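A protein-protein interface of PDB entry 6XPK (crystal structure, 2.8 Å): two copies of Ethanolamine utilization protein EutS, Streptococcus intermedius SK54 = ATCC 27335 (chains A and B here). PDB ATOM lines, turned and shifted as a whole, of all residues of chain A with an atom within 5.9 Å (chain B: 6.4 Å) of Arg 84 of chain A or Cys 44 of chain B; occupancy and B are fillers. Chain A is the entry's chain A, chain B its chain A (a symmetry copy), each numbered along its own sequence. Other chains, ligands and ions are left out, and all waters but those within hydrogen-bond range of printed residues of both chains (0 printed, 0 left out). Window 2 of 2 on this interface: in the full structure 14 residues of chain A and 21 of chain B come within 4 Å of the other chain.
O of Val 82 of chain A is in hydrogen-bond range of SG of Cys 44 of chain B (3.4 Å).
The backbone NH (N) of Met 90 of chain B sits at hydrogen-bond distance from the backbone carbonyl oxygen (O) of Phe 81 of chain B (3.1 Å).
N of Cys 80 of chain B is in hydrogen-bond range of O of Met 90 of chain B.
N of Glu 62 of chain A sits at hydrogen-bond distance from O of Arg 84 of chain A.
Glu 62 of chain A touches Phe 81 of chain B (CB to CZ, 3.97 Å).
Met 90 of chain B touches Glu 62 of chain A (CE to O, 3.2 Å).
Ile 65 of chain A touches Val 41 of chain B (CG1 to CG1, 3.7 Å).
CD1 of Ile 65 of chain A touches SG of Cys 44 of chain B, 3.5 Å away.
CE of Met 90 of chain B touches CG2 of Ile 65 of chain A (3.4 Å).
Cys 44 of chain B touches Arg 84 of chain A (O to NH1, 3.8 Å).
Arg 84 of chain A touches Leu 45 of chain B (NH1 to CD2, 3.9 Å).
Phe 81 of chain B touches Arg 84 of chain A (CD1 to NE, 3.3 Å).
Of the printed residues of chain B, Glu 62 of chain A touches Phe 81 and Met 90.
Ala 64 of chain A touches none of the printed residues of chain B.
Printed residues of chain B within 4 Å of Val 82 of chain A: Cys 44 (3.4 Å).
Arg 84 of chain A touches just these residues of chain B: Cys 44 (3.8 Å), Leu 45 (3.9 Å) and Phe 81 (3.3 Å).
Cys 44 of chain B touches just these residues of chain A: Ile 65 (3.5 Å), Val 82 (3.4 Å) and Arg 84 (3.8 Å).
Printed residues of chain A within 4 Å of Leu 45 of chain B: Arg 84.
Val 47 of chain B touches none of the printed residues of chain A.
Of the printed residues of chain A, Met 90 of chain B touches Glu 62 (3.2 Å) and Ile 65 (3.4 Å).
The nearest printed residue of chain B that does not touch Val 82 of chain A is Ala 40 of chain B (4.8 Å).
Of the 12 printed residues of chain B, 5 touch a printed residue of chain A.
Printed residues of chain B that touch a printed residue of chain A: Val 41, Cys 44, Leu 45, Phe 81 and Met 90.
Hydrophobic or aromatic side chains of chain B that line the printed part of chain A: Val 41, Leu 45, Phe 81 and Met 90.
Among the printed residues, no Asp or Glu carboxylate lies within 4 Å of a Lys or Arg side-chain nitrogen of the other chain.
No position is printed for both chains.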
ATOM      1  N   ASN A  61      -7.645   2.918  24.697  1.00  0.00           N
ATOM      2  CA  ASN A  61      -8.452   3.441  23.560  1.00  0.00           C
ATOM      3  C   ASN A  61      -7.657   3.365  22.248  1.00  0.00           C
ATOM      4  O   ASN A  61      -8.297   3.283  21.183  1.00  0.00           O
ATOM      5  CB  ASN A  61      -8.921   4.875  23.824  1.00  0.00           C
ATOM      6  CG  ASN A  61      -9.796   5.001  25.055  1.00  0.00           C
ATOM      7  OD1 ASN A  61     -10.515   4.071  25.414  1.00  0.00           O
ATOM      8  ND2 ASN A  61      -9.743   6.151  25.707  1.00  0.00           N
ATOM      9  N   GLU A  62      -6.323   3.393  22.319  1.00  0.00           N
ATOM     10  CA  GLU A  62      -5.422   3.462  21.135  1.00  0.00           C
ATOM     11  C   GLU A  62      -5.461   2.139  20.355  1.00  0.00           C
ATOM     12  O   GLU A  62      -5.214   2.176  19.133  1.00  0.00           O
ATOM     13  CB  GLU A  62      -3.998   3.803  21.582  1.00  0.00           C
ATOM     14  CG  GLU A  62      -3.186   2.600  22.026  1.00  0.00           C
ATOM     15  CD  GLU A  62      -2.060   2.930  22.986  1.00  0.00           C
ATOM     16  OE1 GLU A  62      -2.349   3.110  24.184  1.00  0.00           O
ATOM     17  OE2 GLU A  62      -0.903   3.020  22.532  1.00  0.00           O
ATOM     18  N   THR A  63      -5.762   1.021  21.026  1.00  0.00           N
ATOM     19  CA  THR A  63      -5.699  -0.355  20.459  1.00  0.00           C
ATOM     20  C   THR A  63      -6.896  -0.613  19.532  1.00  0.00           C
ATOM     21  O   THR A  63      -6.987  -1.735  18.999  1.00  0.00           O
ATOM     22  CB  THR A  63      -5.576  -1.403  21.573  1.00  0.00           C
ATOM     23  OG1 THR A  63      -6.676  -1.285  22.470  1.00  0.00           O
ATOM     24  CG2 THR A  63      -4.306  -1.255  22.378  1.00  0.00           C
ATOM     25  N   ALA A  64      -7.773   0.383  19.343  1.00  0.00           N
ATOM     26  CA  ALA A  64      -8.809   0.419  18.282  1.00  0.00           C
ATOM     27  C   ALA A  64      -8.135   0.308  16.909  1.00  0.00           C
ATOM     28  O   ALA A  64      -8.765  -0.234  15.980  1.00  0.00           O
ATOM     29  CB  ALA A  64      -9.620   1.688  18.392  1.00  0.00           C
ATOM     30  N   ILE A  65      -6.898   0.806  16.796  1.00  0.00           N
ATOM     31  CA  ILE A  65      -6.071   0.774  15.552  1.00  0.00           C
ATOM     32  C   ILE A  65      -5.687  -0.681  15.242  1.00  0.00           C
ATOM     33  O   ILE A  65      -5.667  -1.039  14.048  1.00  0.00           O
ATOM     34  CB  ILE A  65      -4.843   1.702  15.690  1.00  0.00           C
ATOM     35  CG1 ILE A  65      -4.541   2.433  14.380  1.00  0.00           C
ATOM     36  CG2 ILE A  65      -3.623   0.958  16.216  1.00  0.00           C
ATOM     37  CD1 ILE A  65      -5.462   3.599  14.102  1.00  0.00           C
ATOM     38  N   VAL A  82     -12.624   4.421  12.841  1.00  0.00           N
ATOM     39  CA  VAL A  82     -11.678   4.004  13.918  1.00  0.00           C
ATOM     40  C   VAL A  82     -11.386   5.234  14.786  1.00  0.00           C
ATOM     41  O   VAL A  82     -10.721   6.163  14.285  1.00  0.00           O
ATOM     42  CB  VAL A  82     -10.377   3.404  13.346  1.00  0.00           C
ATOM     43  CG1 VAL A  82      -9.528   2.765  14.436  1.00  0.00           C
ATOM     44  CG2 VAL A  82     -10.648   2.403  12.233  1.00  0.00           C
ATOM     45  N   ASP A  83     -11.883   5.241  16.028  1.00  0.00           N
ATOM     46  CA  ASP A  83     -11.674   6.332  17.018  1.00  0.00           C
ATOM     47  C   ASP A  83     -10.662   5.848  18.064  1.00  0.00           C
ATOM     48  O   ASP A  83     -11.022   4.964  18.867  1.00  0.00           O
ATOM     49  CB  ASP A  83     -13.003   6.761  17.645  1.00  0.00           C
ATOM     50  CG  ASP A  83     -12.955   8.110  18.346  1.00  0.00           C
ATOM     51  OD1 ASP A  83     -11.854   8.518  18.768  1.00  0.00           O
ATOM     52  OD2 ASP A  83     -14.023   8.743  18.462  1.00  0.00           O
ATOM     53  N   ARG A  84      -9.446   6.408  18.045  1.00  0.00           N
ATOM     54  CA  ARG A  84      -8.318   6.004  18.930  1.00  0.00           C
ATOM     55  C   ARG A  84      -8.423   6.729  20.280  1.00  0.00           C
ATOM     56  O   ARG A  84      -7.699   6.331  21.212  1.00  0.00           O
ATOM     57  CB  ARG A  84      -6.972   6.272  18.245  1.00  0.00           C
ATOM     58  CG  ARG A  84      -6.429   7.688  18.398  1.00  0.00           C
ATOM     59  CD  ARG A  84      -4.917   7.712  18.270  1.00  0.00           C
ATOM     60  NE  ARG A  84      -4.362   9.059  18.208  1.00  0.00           N
ATOM     61  CZ  ARG A  84      -4.340   9.832  17.122  1.00  0.00           C
ATOM     62  NH1 ARG A  84      -4.856   9.407  15.980  1.00  0.00           N
ATOM     63  NH2 ARG A  84      -3.802  11.038  17.187  1.00  0.00           N
ATOM     64  N   PHE A  85      -9.281   7.751  20.376  1.00  0.00           N
ATOM     65  CA  PHE A  85      -9.466   8.597  21.586  1.00  0.00           C
ATOM     66  C   PHE A  85     -10.477   7.937  22.533  1.00  0.00           C
ATOM     67  O   PHE A  85     -10.228   7.932  23.753  1.00  0.00           O
ATOM     68  CB  PHE A  85      -9.901  10.010  21.190  1.00  0.00           C
ATOM     69  CG  PHE A  85      -8.977  10.696  20.215  1.00  0.00           C
ATOM     70  CD1 PHE A  85      -7.726  11.139  20.614  1.00  0.00           C
ATOM     71  CD2 PHE A  85      -9.355  10.892  18.894  1.00  0.00           C
ATOM     72  CE1 PHE A  85      -6.874  11.765  19.717  1.00  0.00           C
ATOM     73  CE2 PHE A  85      -8.502  11.519  17.998  1.00  0.00           C
ATOM     74  CZ  PHE A  85      -7.263  11.955  18.410  1.00  0.00           C
ATOM     75  N   THR A  86     -11.575   7.404  21.986  1.00  0.00           N
ATOM     76  CA  THR A  86     -12.673   6.738  22.740  1.00  0.00           C
ATOM     77  C   THR A  86     -12.440   5.222  22.801  1.00  0.00           C
ATOM     78  O   THR A  86     -12.945   4.594  23.754  1.00  0.00           O
ATOM     79  CB  THR A  86     -14.041   7.059  22.125  1.00  0.00           C
ATOM     80  OG1 THR A  86     -14.068   6.532  20.798  1.00  0.00           O
ATOM     81  CG2 THR A  86     -14.339   8.541  22.093  1.00  0.00           C
ATOM     82  N   GLY A  87     -11.716   4.658  21.827  1.00  0.00           N
ATOM     83  CA  GLY A  87     -11.443   3.211  21.726  1.00  0.00           C
ATOM     84  C   GLY A  87     -12.598   2.479  21.069  1.00  0.00           C
ATOM     85  O   GLY A  87     -13.091   1.502  21.663  1.00  0.00           O
ATOM     86  N   SER A  88     -12.998   2.935  19.878  1.00  0.00           N
ATOM     87  CA  SER A  88     -14.206   2.486  19.139  1.00  0.00           C
ATOM     88  C   SER A  88     -13.830   2.090  17.707  1.00  0.00           C
ATOM     89  O   SER A  88     -13.053   2.832  17.074  1.00  0.00           O
ATOM     90  CB  SER A  88     -15.253   3.568  19.147  1.00  0.00           C
ATOM     91  OG  SER A  88     -15.551   3.974  20.475  1.00  0.00           O
ATOM     92  N   GLU B  39      -5.227   1.028   4.570  1.00  0.00           N
ATOM     93  CA  GLU B  39      -5.677   2.407   4.227  1.00  0.00           C
ATOM     94  C   GLU B  39      -6.316   3.088   5.446  1.00  0.00           C
ATOM     95  O   GLU B  39      -5.819   4.159   5.845  1.00  0.00           O
ATOM     96  CB  GLU B  39      -6.666   2.348   3.058  1.00  0.00           C
ATOM     97  CG  GLU B  39      -7.295   3.689   2.708  1.00  0.00           C
ATOM     98  CD  GLU B  39      -8.103   3.699   1.419  1.00  0.00           C
ATOM     99  OE1 GLU B  39      -9.141   4.390   1.382  1.00  0.00           O
ATOM    100  OE2 GLU B  39      -7.690   3.025   0.454  1.00  0.00           O
ATOM    101  N   ALA B  40      -7.382   2.495   5.996  1.00  0.00           N
ATOM    102  CA  ALA B  40      -8.205   3.048   7.101  1.00  0.00           C
ATOM    103  C   ALA B  40      -7.337   3.318   8.339  1.00  0.00           C
ATOM    104  O   ALA B  40      -7.589   4.332   9.019  1.00  0.00           O
ATOM    105  CB  ALA B  40      -9.339   2.105   7.420  1.00  0.00           C
ATOM    106  N   VAL B  41      -6.363   2.444   8.618  1.00  0.00           N
ATOM    107  CA  VAL B  41      -5.423   2.558   9.776  1.00  0.00           C
ATOM    108  C   VAL B  41      -4.455   3.721   9.523  1.00  0.00           C
ATOM    109  O   VAL B  41      -4.232   4.513  10.459  1.00  0.00           O
ATOM    110  CB  VAL B  41      -4.672   1.235  10.023  1.00  0.00           C
ATOM    111  CG1 VAL B  41      -3.527   1.403  11.012  1.00  0.00           C
ATOM    112  CG2 VAL B  41      -5.618   0.132  10.478  1.00  0.00           C
ATOM    113  N   TYR B  42      -3.890   3.803   8.312  1.00  0.00           N
ATOM    114  CA  TYR B  42      -2.984   4.896   7.868  1.00  0.00           C
ATOM    115  C   TYR B  42      -3.735   6.233   7.907  1.00  0.00           C
ATOM    116  O   TYR B  42      -3.227   7.187   8.528  1.00  0.00           O
ATOM    117  CB  TYR B  42      -2.455   4.643   6.454  1.00  0.00           C
ATOM    118  CG  TYR B  42      -1.453   3.523   6.315  1.00  0.00           C
ATOM    119  CD1 TYR B  42      -0.351   3.430   7.151  1.00  0.00           C
ATOM    120  CD2 TYR B  42      -1.580   2.579   5.306  1.00  0.00           C
ATOM    121  CE1 TYR B  42       0.581   2.413   7.010  1.00  0.00           C
ATOM    122  CE2 TYR B  42      -0.655   1.558   5.150  1.00  0.00           C
ATOM    123  CZ  TYR B  42       0.430   1.475   6.005  1.00  0.00           C
ATOM    124  OH  TYR B  42       1.341   0.470   5.854  1.00  0.00           O
ATOM    125  N   GLU B  43      -4.904   6.284   7.258  1.00  0.00           N
ATOM    126  CA  GLU B  43      -5.773   7.488   7.141  1.00  0.00           C
ATOM    127  C   GLU B  43      -6.146   8.001   8.538  1.00  0.00           C
ATOM    128  O   GLU B  43      -6.207   9.235   8.714  1.00  0.00           O
ATOM    129  CB  GLU B  43      -7.030   7.163   6.333  1.00  0.00           C
ATOM    130  N   CYS B  44      -6.388   7.086   9.485  1.00  0.00           N
ATOM    131  CA  CYS B  44      -6.744   7.377  10.902  1.00  0.00           C
ATOM    132  C   CYS B  44      -5.600   8.132  11.592  1.00  0.00           C
ATOM    133  O   CYS B  44      -5.894   9.100  12.321  1.00  0.00           O
ATOM    134  CB  CYS B  44      -7.062   6.094  11.662  1.00  0.00           C
ATOM    135  SG  CYS B  44      -7.449   6.357  13.412  1.00  0.00           S
ATOM    136  N   LEU B  45      -4.352   7.706  11.367  1.00  0.00           N
ATOM    137  CA  LEU B  45      -3.136   8.280  12.007  1.00  0.00           C
ATOM    138  C   LEU B  45      -2.600   9.459  11.184  1.00  0.00           C
ATOM    139  O   LEU B  45      -2.042  10.390  11.796  1.00  0.00           O
ATOM    140  CB  LEU B  45      -2.074   7.184  12.161  1.00  0.00           C
ATOM    141  CG  LEU B  45      -2.298   6.207  13.314  1.00  0.00           C
ATOM    142  CD1 LEU B  45      -1.346   5.026  13.216  1.00  0.00           C
ATOM    143  CD2 LEU B  45      -2.146   6.902  14.659  1.00  0.00           C
ATOM    144  N   GLY B  46      -2.759   9.419   9.856  1.00  0.00           N
ATOM    145  CA  GLY B  46      -2.265  10.452   8.923  1.00  0.00           C
ATOM    146  C   GLY B  46      -0.818  10.199   8.527  1.00  0.00           C
ATOM    147  O   GLY B  46      -0.001  11.133   8.646  1.00  0.00           O
ATOM    148  N   VAL B  47      -0.525   8.975   8.073  1.00  0.00           N
ATOM    149  CA  VAL B  47       0.830   8.488   7.673  1.00  0.00           C
ATOM    150  C   VAL B  47       0.885   8.425   6.138  1.00  0.00           C
ATOM    151  O   VAL B  47      -0.192   8.496   5.511  1.00  0.00           O
ATOM    152  CB  VAL B  47       1.124   7.122   8.332  1.00  0.00           C
ATOM    153  CG1 VAL B  47       2.431   6.496   7.867  1.00  0.00           C
ATOM    154  CG2 VAL B  47       1.109   7.228   9.850  1.00  0.00           C
ATOM    155  N   CYS B  80       3.823   9.482  15.725  1.00  0.00           N
ATOM    156  CA  CYS B  80       2.418   9.730  15.298  1.00  0.00           C
ATOM    157  C   CYS B  80       1.707  10.594  16.346  1.00  0.00           C
ATOM    158  O   CYS B  80       1.255  11.699  15.986  1.00  0.00           O
ATOM    159  CB  CYS B  80       1.651   8.428  15.098  1.00  0.00           C
ATOM    160  SG  CYS B  80       2.285   7.416  13.734  1.00  0.00           S
ATOM    161  N   PHE B  81       1.613  10.100  17.585  1.00  0.00           N
ATOM    162  CA  PHE B  81       1.005  10.814  18.739  1.00  0.00           C
ATOM    163  C   PHE B  81       1.638  10.319  20.046  1.00  0.00           C
ATOM    164  O   PHE B  81       2.004   9.128  20.133  1.00  0.00           O
ATOM    165  CB  PHE B  81      -0.518  10.648  18.735  1.00  0.00           C
ATOM    166  CG  PHE B  81      -1.043   9.411  19.422  1.00  0.00           C
ATOM    167  CD1 PHE B  81      -1.256   8.239  18.714  1.00  0.00           C
ATOM    168  CD2 PHE B  81      -1.343   9.425  20.777  1.00  0.00           C
ATOM    169  CE1 PHE B  81      -1.745   7.106  19.349  1.00  0.00           C
ATOM    170  CE2 PHE B  81      -1.830   8.291  21.409  1.00  0.00           C
ATOM    171  CZ  PHE B  81      -2.031   7.133  20.694  1.00  0.00           C
ATOM    172  N   MET B  90       2.499   6.075  19.660  1.00  0.00           N
ATOM    173  CA  MET B  90       2.462   5.433  18.319  1.00  0.00           C
ATOM    174  C   MET B  90       3.473   6.123  17.400  1.00  0.00           C
ATOM    175  O   MET B  90       3.695   7.339  17.564  1.00  0.00           O
ATOM    176  CB  MET B  90       1.067   5.510  17.693  1.00  0.00           C
ATOM    177  CG  MET B  90       0.117   4.449  18.209  1.00  0.00           C
ATOM    178  SD  MET B  90      -1.265   4.161  17.078  1.00  0.00           S
ATOM    179  CE  MET B  90      -2.475   3.483  18.210  1.00  0.00           C
